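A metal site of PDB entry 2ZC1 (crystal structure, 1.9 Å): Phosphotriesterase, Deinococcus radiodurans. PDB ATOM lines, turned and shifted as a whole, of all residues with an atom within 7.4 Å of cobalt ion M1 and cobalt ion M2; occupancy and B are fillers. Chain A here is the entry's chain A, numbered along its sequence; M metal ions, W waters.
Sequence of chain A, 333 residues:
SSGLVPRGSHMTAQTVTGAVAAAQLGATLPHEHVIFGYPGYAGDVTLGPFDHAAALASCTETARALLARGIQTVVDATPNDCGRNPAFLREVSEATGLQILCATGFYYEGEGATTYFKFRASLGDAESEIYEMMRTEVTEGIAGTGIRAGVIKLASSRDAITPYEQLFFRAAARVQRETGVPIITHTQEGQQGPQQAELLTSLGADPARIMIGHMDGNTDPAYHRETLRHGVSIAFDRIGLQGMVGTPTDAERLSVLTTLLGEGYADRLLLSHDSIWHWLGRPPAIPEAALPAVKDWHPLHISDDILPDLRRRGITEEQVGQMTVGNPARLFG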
ATOM      1  N   HIS A  31      18.998  12.748  16.888  1.00  0.00           N
ATOM      2  CA  HIS A  31      18.164  13.812  16.322  1.00  0.00           C
ATOM      3  C   HIS A  31      17.951  13.636  14.813  1.00  0.00           C
ATOM      4  O   HIS A  31      18.791  14.059  14.018  1.00  0.00           O
ATOM      5  CB  HIS A  31      18.802  15.203  16.569  1.00  0.00           C
ATOM      6  CG  HIS A  31      17.898  16.351  16.206  1.00  0.00           C
ATOM      7  ND1 HIS A  31      17.607  17.378  17.088  1.00  0.00           N
ATOM      8  CD2 HIS A  31      17.237  16.643  15.062  1.00  0.00           C
ATOM      9  CE1 HIS A  31      16.792  18.245  16.505  1.00  0.00           C
ATOM     10  NE2 HIS A  31      16.555  17.821  15.269  1.00  0.00           N
ATOM     11  N   GLU A  32      16.852  12.997  14.446  1.00  0.00           N
ATOM     12  CA  GLU A  32      16.498  12.804  13.034  1.00  0.00           C
ATOM     13  C   GLU A  32      14.987  12.989  12.903  1.00  0.00           C
ATOM     14  O   GLU A  32      14.260  13.113  13.898  1.00  0.00           O
ATOM     15  CB  GLU A  32      16.871  11.392  12.574  1.00  0.00           C
ATOM     16  CG  GLU A  32      18.303  10.949  12.919  1.00  0.00           C
ATOM     17  CD  GLU A  32      19.354  11.660  12.106  1.00  0.00           C
ATOM     18  OE1 GLU A  32      19.021  12.198  11.018  1.00  0.00           O
ATOM     19  OE2 GLU A  32      20.520  11.655  12.536  1.00  0.00           O
ATOM     20  N   HIS A  33      14.505  12.990  11.654  1.00  0.00           N
ATOM     21  CA  HIS A  33      13.075  13.115  11.402  1.00  0.00           C
ATOM     22  C   HIS A  33      12.646  12.084  10.371  1.00  0.00           C
ATOM     23  O   HIS A  33      13.009  12.190   9.215  1.00  0.00           O
ATOM     24  CB  HIS A  33      12.765  14.522  10.869  1.00  0.00           C
ATOM     25  CG  HIS A  33      13.072  15.609  11.845  1.00  0.00           C
ATOM     26  ND1 HIS A  33      12.267  15.870  12.931  1.00  0.00           N
ATOM     27  CD2 HIS A  33      14.133  16.450  11.946  1.00  0.00           C
ATOM     28  CE1 HIS A  33      12.817  16.820  13.659  1.00  0.00           C
ATOM     29  NE2 HIS A  33      13.950  17.175  13.097  1.00  0.00           N
ATOM     30  N   PHE A  36       8.504  14.856   8.238  1.00  0.00           N
ATOM     31  CA  PHE A  36       8.502  16.235   8.725  1.00  0.00           C
ATOM     32  C   PHE A  36       7.731  17.145   7.760  1.00  0.00           C
ATOM     33  O   PHE A  36       7.788  16.982   6.546  1.00  0.00           O
ATOM     34  CB  PHE A  36       9.946  16.713   8.856  1.00  0.00           C
ATOM     35  CG  PHE A  36      10.088  18.103   9.422  1.00  0.00           C
ATOM     36  CD1 PHE A  36       9.909  19.228   8.614  1.00  0.00           C
ATOM     37  CD2 PHE A  36      10.397  18.277  10.763  1.00  0.00           C
ATOM     38  CE1 PHE A  36      10.025  20.520   9.147  1.00  0.00           C
ATOM     39  CE2 PHE A  36      10.521  19.566  11.312  1.00  0.00           C
ATOM     40  CZ  PHE A  36      10.326  20.684  10.504  1.00  0.00           C
ATOM     41  N   ALA A  77      13.060  13.729  16.493  1.00  0.00           N
ATOM     42  CA  ALA A  77      12.905  14.997  17.168  1.00  0.00           C
ATOM     43  C   ALA A  77      11.800  15.909  16.667  1.00  0.00           C
ATOM     44  O   ALA A  77      11.765  17.086  17.021  1.00  0.00           O
ATOM     45  CB  ALA A  77      14.217  15.682  17.127  1.00  0.00           C
ATOM     46  N   THR A  78      10.876  15.370  15.878  1.00  0.00           N
ATOM     47  CA  THR A  78       9.796  16.134  15.279  1.00  0.00           C
ATOM     48  C   THR A  78       8.803  16.717  16.282  1.00  0.00           C
ATOM     49  O   THR A  78       8.145  15.972  16.994  1.00  0.00           O
ATOM     50  CB  THR A  78       9.002  15.266  14.274  1.00  0.00           C
ATOM     51  OG1 THR A  78       9.923  14.533  13.463  1.00  0.00           O
ATOM     52  CG2 THR A  78       8.083  16.129  13.397  1.00  0.00           C
ATOM     53  N   PRO A  79       8.677  18.070  16.327  1.00  0.00           N
ATOM     54  CA  PRO A  79       7.769  18.807  17.210  1.00  0.00           C
ATOM     55  C   PRO A  79       6.335  18.458  16.844  1.00  0.00           C
ATOM     56  O   PRO A  79       6.057  18.090  15.695  1.00  0.00           O
ATOM     57  CB  PRO A  79       8.058  20.267  16.881  1.00  0.00           C
ATOM     58  CG  PRO A  79       9.462  20.260  16.457  1.00  0.00           C
ATOM     59  CD  PRO A  79       9.586  18.990  15.615  1.00  0.00           C
ATOM     60  N   TYR A 107       7.663  23.731  18.060  1.00  0.00           N
ATOM     61  CA  TYR A 107       8.860  24.320  17.489  1.00  0.00           C
ATOM     62  C   TYR A 107       9.080  25.753  17.943  1.00  0.00           C
ATOM     63  O   TYR A 107       8.223  26.347  18.604  1.00  0.00           O
ATOM     64  CB  TYR A 107       8.845  24.195  15.946  1.00  0.00           C
ATOM     65  CG  TYR A 107      10.215  23.929  15.341  1.00  0.00           C
ATOM     66  CD1 TYR A 107      11.238  23.386  16.117  1.00  0.00           C
ATOM     67  CD2 TYR A 107      10.479  24.196  14.002  1.00  0.00           C
ATOM     68  CE1 TYR A 107      12.487  23.110  15.572  1.00  0.00           C
ATOM     69  CE2 TYR A 107      11.746  23.907  13.447  1.00  0.00           C
ATOM     70  CZ  TYR A 107      12.736  23.369  14.234  1.00  0.00           C
ATOM     71  OH  TYR A 107      13.962  23.033  13.693  1.00  0.00           O
ATOM     72  N   TYR A 108      10.229  26.324  17.590  1.00  0.00           N
ATOM     73  CA  TYR A 108      10.557  27.684  17.992  1.00  0.00           C
ATOM     74  C   TYR A 108       9.649  28.705  17.300  1.00  0.00           C
ATOM     75  O   TYR A 108       9.015  28.405  16.291  1.00  0.00           O
ATOM     76  CB  TYR A 108      12.045  27.968  17.767  1.00  0.00           C
ATOM     77  CG  TYR A 108      12.468  28.269  16.351  1.00  0.00           C
ATOM     78  CD1 TYR A 108      12.482  27.272  15.361  1.00  0.00           C
ATOM     79  CD2 TYR A 108      12.873  29.555  15.992  1.00  0.00           C
ATOM     80  CE1 TYR A 108      12.898  27.568  14.039  1.00  0.00           C
ATOM     81  CE2 TYR A 108      13.284  29.863  14.675  1.00  0.00           C
ATOM     82  CZ  TYR A 108      13.292  28.867  13.720  1.00  0.00           C
ATOM     83  OH  TYR A 108      13.735  29.164  12.450  1.00  0.00           O
ATOM     84  N   GLU A 111       9.476  29.380  13.282  1.00  0.00           N
ATOM     85  CA  GLU A 111       8.929  28.445  12.312  1.00  0.00           C
ATOM     86  C   GLU A 111       7.764  27.598  12.799  1.00  0.00           C
ATOM     87  O   GLU A 111       7.152  26.889  12.003  1.00  0.00           O
ATOM     88  CB  GLU A 111      10.020  27.489  11.809  1.00  0.00           C
ATOM     89  CG  GLU A 111      10.913  28.068  10.739  1.00  0.00           C
ATOM     90  CD  GLU A 111      12.066  27.139  10.371  1.00  0.00           C
ATOM     91  OE1 GLU A 111      11.961  25.908  10.585  1.00  0.00           O
ATOM     92  OE2 GLU A 111      13.076  27.642   9.858  1.00  0.00           O
ATOM     93  N   KCX A 153      11.024  17.874  23.264  1.00  0.00           N
ATOM     94  CA  KCX A 153      11.775  18.690  22.311  1.00  0.00           C
ATOM     95  CB  KCX A 153      11.375  18.343  20.863  1.00  0.00           C
ATOM     96  CG  KCX A 153      11.863  19.307  19.764  1.00  0.00           C
ATOM     97  CD  KCX A 153      13.372  19.299  19.607  1.00  0.00           C
ATOM     98  CE  KCX A 153      13.828  20.188  18.449  1.00  0.00           C
ATOM     99  NZ  KCX A 153      13.522  19.578  17.146  1.00  0.00           N
ATOM    100  C   KCX A 153      11.484  20.160  22.619  1.00  0.00           C
ATOM    101  O   KCX A 153      10.331  20.566  22.695  1.00  0.00           O
ATOM    102  CX  KCX A 153      14.083  19.931  15.980  1.00  0.00           C
ATOM    103  OQ1 KCX A 153      14.902  20.885  15.900  1.00  0.00           O
ATOM    104  OQ2 KCX A 153      13.773  19.346  14.917  1.00  0.00           O
ATOM    105  N   LEU A 154      12.533  20.923  22.807  1.00  0.00           N
ATOM    106  CA  LEU A 154      12.458  22.347  23.058  1.00  0.00           C
ATOM    107  C   LEU A 154      13.206  23.044  21.934  1.00  0.00           C
ATOM    108  O   LEU A 154      14.129  22.465  21.352  1.00  0.00           O
ATOM    109  CB  LEU A 154      13.154  22.688  24.387  1.00  0.00           C
ATOM    110  CG  LEU A 154      12.454  22.204  25.658  1.00  0.00           C
ATOM    111  CD1 LEU A 154      13.288  22.612  26.881  1.00  0.00           C
ATOM    112  CD2 LEU A 154      11.061  22.845  25.738  1.00  0.00           C
ATOM    113  N   ALA A 155      12.847  24.300  21.667  1.00  0.00           N
ATOM    114  CA  ALA A 155      13.510  25.050  20.608  1.00  0.00           C
ATOM    115  C   ALA A 155      13.437  26.540  20.859  1.00  0.00           C
ATOM    116  O   ALA A 155      12.420  27.049  21.290  1.00  0.00           O
ATOM    117  CB  ALA A 155      12.853  24.732  19.261  1.00  0.00           C
ATOM    118  N   THR A 185      17.176  19.729  22.405  1.00  0.00           N
ATOM    119  CA  THR A 185      16.765  21.015  21.927  1.00  0.00           C
ATOM    120  C   THR A 185      17.289  21.447  20.562  1.00  0.00           C
ATOM    121  O   THR A 185      18.236  20.886  20.028  1.00  0.00           O
ATOM    122  CB  THR A 185      17.191  22.132  22.918  1.00  0.00           C
ATOM    123  OG1 THR A 185      18.557  22.499  22.655  1.00  0.00           O
ATOM    124  CG2 THR A 185      17.083  21.642  24.369  1.00  0.00           C
ATOM    125  N   HIS A 186      16.644  22.476  20.057  1.00  0.00           N
ATOM    126  CA  HIS A 186      17.010  23.140  18.824  1.00  0.00           C
ATOM    127  C   HIS A 186      17.553  24.514  19.229  1.00  0.00           C
ATOM    128  O   HIS A 186      16.952  25.187  20.077  1.00  0.00           O
ATOM    129  CB  HIS A 186      15.757  23.331  17.955  1.00  0.00           C
ATOM    130  CG  HIS A 186      15.874  24.446  16.949  1.00  0.00           C
ATOM    131  ND1 HIS A 186      15.903  24.209  15.590  1.00  0.00           N
ATOM    132  CD2 HIS A 186      15.888  25.792  17.098  1.00  0.00           C
ATOM    133  CE1 HIS A 186      15.913  25.367  14.945  1.00  0.00           C
ATOM    134  NE2 HIS A 186      15.905  26.344  15.839  1.00  0.00           N
ATOM    135  N   THR A 187      18.694  24.908  18.680  1.00  0.00           N
ATOM    136  CA  THR A 187      19.199  26.254  18.885  1.00  0.00           C
ATOM    137  C   THR A 187      19.229  26.804  17.468  1.00  0.00           C
ATOM    138  O   THR A 187      19.556  26.083  16.505  1.00  0.00           O
ATOM    139  CB  THR A 187      20.643  26.331  19.451  1.00  0.00           C
ATOM    140  OG1 THR A 187      21.535  25.565  18.631  1.00  0.00           O
ATOM    141  CG2 THR A 187      20.669  25.855  20.914  1.00  0.00           C
ATOM    142  N   GLN A 188      18.876  28.072  17.337  1.00  0.00           N
ATOM    143  CA  GLN A 188      18.824  28.715  16.033  1.00  0.00           C
ATOM    144  C   GLN A 188      20.087  29.479  15.648  1.00  0.00           C
ATOM    145  O   GLN A 188      20.539  30.354  16.372  1.00  0.00           O
ATOM    146  CB  GLN A 188      17.613  29.643  15.994  1.00  0.00           C
ATOM    147  CG  GLN A 188      17.402  30.355  14.689  1.00  0.00           C
ATOM    148  CD  GLN A 188      16.978  29.444  13.555  1.00  0.00           C
ATOM    149  OE1 GLN A 188      17.098  29.816  12.382  1.00  0.00           O
ATOM    150  NE2 GLN A 188      16.462  28.262  13.894  1.00  0.00           N
ATOM    151  N   GLY A 213      20.989  21.020  21.345  1.00  0.00           N
ATOM    152  CA  GLY A 213      21.298  20.695  19.961  1.00  0.00           C
ATOM    153  C   GLY A 213      21.704  21.809  19.023  1.00  0.00           C
ATOM    154  O   GLY A 213      21.816  22.985  19.399  1.00  0.00           O
ATOM    155  N   HIS A 214      21.919  21.396  17.767  1.00  0.00           N
ATOM    156  CA  HIS A 214      22.366  22.268  16.671  1.00  0.00           C
ATOM    157  C   HIS A 214      23.568  23.090  17.108  1.00  0.00           C
ATOM    158  O   HIS A 214      23.761  24.223  16.667  1.00  0.00           O
ATOM    159  CB  HIS A 214      21.257  23.206  16.208  1.00  0.00           C
ATOM    160  CG  HIS A 214      19.992  22.508  15.799  1.00  0.00           C
ATOM    161  ND1 HIS A 214      19.926  21.157  15.534  1.00  0.00           N
ATOM    162  CD2 HIS A 214      18.734  22.987  15.638  1.00  0.00           C
ATOM    163  CE1 HIS A 214      18.684  20.836  15.216  1.00  0.00           C
ATOM    164  NE2 HIS A 214      17.942  21.926  15.279  1.00  0.00           N
ATOM    165  N   ASP A 237      24.321  17.948  15.559  1.00  0.00           N
ATOM    166  CA  ASP A 237      23.266  17.155  14.972  1.00  0.00           C
ATOM    167  C   ASP A 237      22.700  17.486  13.609  1.00  0.00           C
ATOM    168  O   ASP A 237      21.624  17.023  13.279  1.00  0.00           O
ATOM    169  CB  ASP A 237      22.110  17.037  15.977  1.00  0.00           C
ATOM    170  CG  ASP A 237      21.643  18.380  16.489  1.00  0.00           C
ATOM    171  OD1 ASP A 237      21.826  19.386  15.754  1.00  0.00           O
ATOM    172  OD2 ASP A 237      21.075  18.456  17.611  1.00  0.00           O
ATOM    173  N   ARG A 238      23.416  18.291  12.823  1.00  0.00           N
ATOM    174  CA  ARG A 238      22.982  18.613  11.468  1.00  0.00           C
ATOM    175  C   ARG A 238      24.170  18.317  10.541  1.00  0.00           C
ATOM    176  O   ARG A 238      24.416  19.055   9.569  1.00  0.00           O
ATOM    177  CB  ARG A 238      22.614  20.082  11.346  1.00  0.00           C
ATOM    178  CG  ARG A 238      21.771  20.571  12.521  1.00  0.00           C
ATOM    179  CD  ARG A 238      21.256  21.948  12.271  1.00  0.00           C
ATOM    180  NE  ARG A 238      20.019  21.889  11.504  1.00  0.00           N
ATOM    181  CZ  ARG A 238      19.663  22.767  10.577  1.00  0.00           C
ATOM    182  NH1 ARG A 238      20.468  23.793  10.279  1.00  0.00           N
ATOM    183  NH2 ARG A 238      18.488  22.638   9.965  1.00  0.00           N
ATOM    184  N   HIS A 273      22.244  13.875  12.158  1.00  0.00           N
ATOM    185  CA  HIS A 273      22.134  14.565  10.878  1.00  0.00           C
ATOM    186  C   HIS A 273      20.969  15.521  10.727  1.00  0.00           C
ATOM    187  O   HIS A 273      21.023  16.381   9.855  1.00  0.00           O
ATOM    188  CB  HIS A 273      21.979  13.548   9.716  1.00  0.00           C
ATOM    189  CG  HIS A 273      22.806  12.300   9.856  1.00  0.00           C
ATOM    190  ND1 HIS A 273      23.982  12.120   9.180  1.00  0.00           N
ATOM    191  CD2 HIS A 273      22.591  11.167  10.564  1.00  0.00           C
ATOM    192  CE1 HIS A 273      24.478  10.926   9.464  1.00  0.00           C
ATOM    193  NE2 HIS A 273      23.649  10.329  10.302  1.00  0.00           N
ATOM    194  N   ASP A 274      19.917  15.342  11.533  1.00  0.00           N
ATOM    195  CA  ASP A 274      18.726  16.177  11.412  1.00  0.00           C
ATOM    196  C   ASP A 274      18.161  15.904  10.011  1.00  0.00           C
ATOM    197  O   ASP A 274      17.638  16.795   9.361  1.00  0.00           O
ATOM    198  CB  ASP A 274      19.088  17.667  11.566  1.00  0.00           C
ATOM    199  CG  ASP A 274      17.886  18.542  11.840  1.00  0.00           C
ATOM    200  OD1 ASP A 274      16.836  17.993  12.230  1.00  0.00           O
ATOM    201  OD2 ASP A 274      17.960  19.774  11.675  1.00  0.00           O
ATOM    202  N   SER A 275      18.259  14.666   9.566  1.00  0.00           N
ATOM    203  CA  SER A 275      17.749  14.307   8.243  1.00  0.00           C
ATOM    204  C   SER A 275      16.226  14.221   8.238  1.00  0.00           C
ATOM    205  O   SER A 275      15.580  14.116   9.292  1.00  0.00           O
ATOM    206  CB  SER A 275      18.341  12.946   7.822  1.00  0.00           C
ATOM    207  OG  SER A 275      17.823  11.900   8.618  1.00  0.00           O
ATOM    208  N   ILE A 276      15.631  14.310   7.059  1.00  0.00           N
ATOM    209  CA  ILE A 276      14.182  14.138   6.953  1.00  0.00           C
ATOM    210  C   ILE A 276      14.037  13.001   5.953  1.00  0.00           C
ATOM    211  O   ILE A 276      14.418  13.136   4.784  1.00  0.00           O
ATOM    212  CB  ILE A 276      13.496  15.427   6.465  1.00  0.00           C
ATOM    213  CG1 ILE A 276      13.501  16.464   7.615  1.00  0.00           C
ATOM    214  CG2 ILE A 276      12.047  15.132   6.023  1.00  0.00           C
ATOM    215  CD1 ILE A 276      13.125  17.869   7.187  1.00  0.00           C
HETATM  216 CO    CO M   1      15.305  18.745  13.681  1.00  0.00          CO
HETATM  217 CO    CO M   2      15.834  22.152  14.570  1.00  0.00          CO
HETATM  218  O   HOH W   1      16.821  23.250  12.766  1.00  0.00           O
HETATM  219  O   HOH W   2      15.892  20.500  13.195  1.00  0.00           O
HETATM  220  O   HOH W   3      13.808  20.487  11.488  1.00  0.00           O
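NZ of KCX 153 lies within hydrogen-bond range of O of Ala 77. O of Ser 275 sits at hydrogen-bond distance from N of His 33, at 2.8 Å. The backbone carbonyl oxygen of His 214 lies within hydrogen-bond range of the side-chain hydroxyl of Thr 187 (3.3 Å). OD1 of Asp 237 is in hydrogen-bond range of ND1 of His 214, at 2.6 Å. The side-chain carboxylate of Asp 274 is in salt-bridge range of the guanidinium group of Arg 238, at 3.0 Å. N of Asp 274 is in hydrogen-bond range of OE1 of Glu 32 (3.3 Å). The backbone NH of Asp 274 lies within hydrogen-bond range of the backbone carbonyl oxygen of Asp 237 (3.0 Å). The backbone carbonyl oxygen (O) of Leu 154 sits at hydrogen-bond distance from the backbone NH (N) of His 186, at 2.8 Å.
Within 4 Å of cobalt ion M1: His 31, His 33, KCX 153 and Asp 274. The nearest printed residue that does not touch cobalt ion M1 is His 214 (4.3 Å).
The nearest printed residue that does not touch cobalt ion M2 is Asp 274 (4.3 Å).
Cobalt ion M1 is bound by water W2, OQ2 of KCX 153, NE2 of His 33, NE2 of His 31 and OD1 of Asp 274. Cobalt ion M1 has five donor atoms within binding distance.
Cobalt ion M2 is bound by OQ1 of KCX 153, water W2, NE2 of His 214, OH of Tyr 107, ND1 of His 186 and water W1. Cobalt ion M2 has six donor atoms within binding distance.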
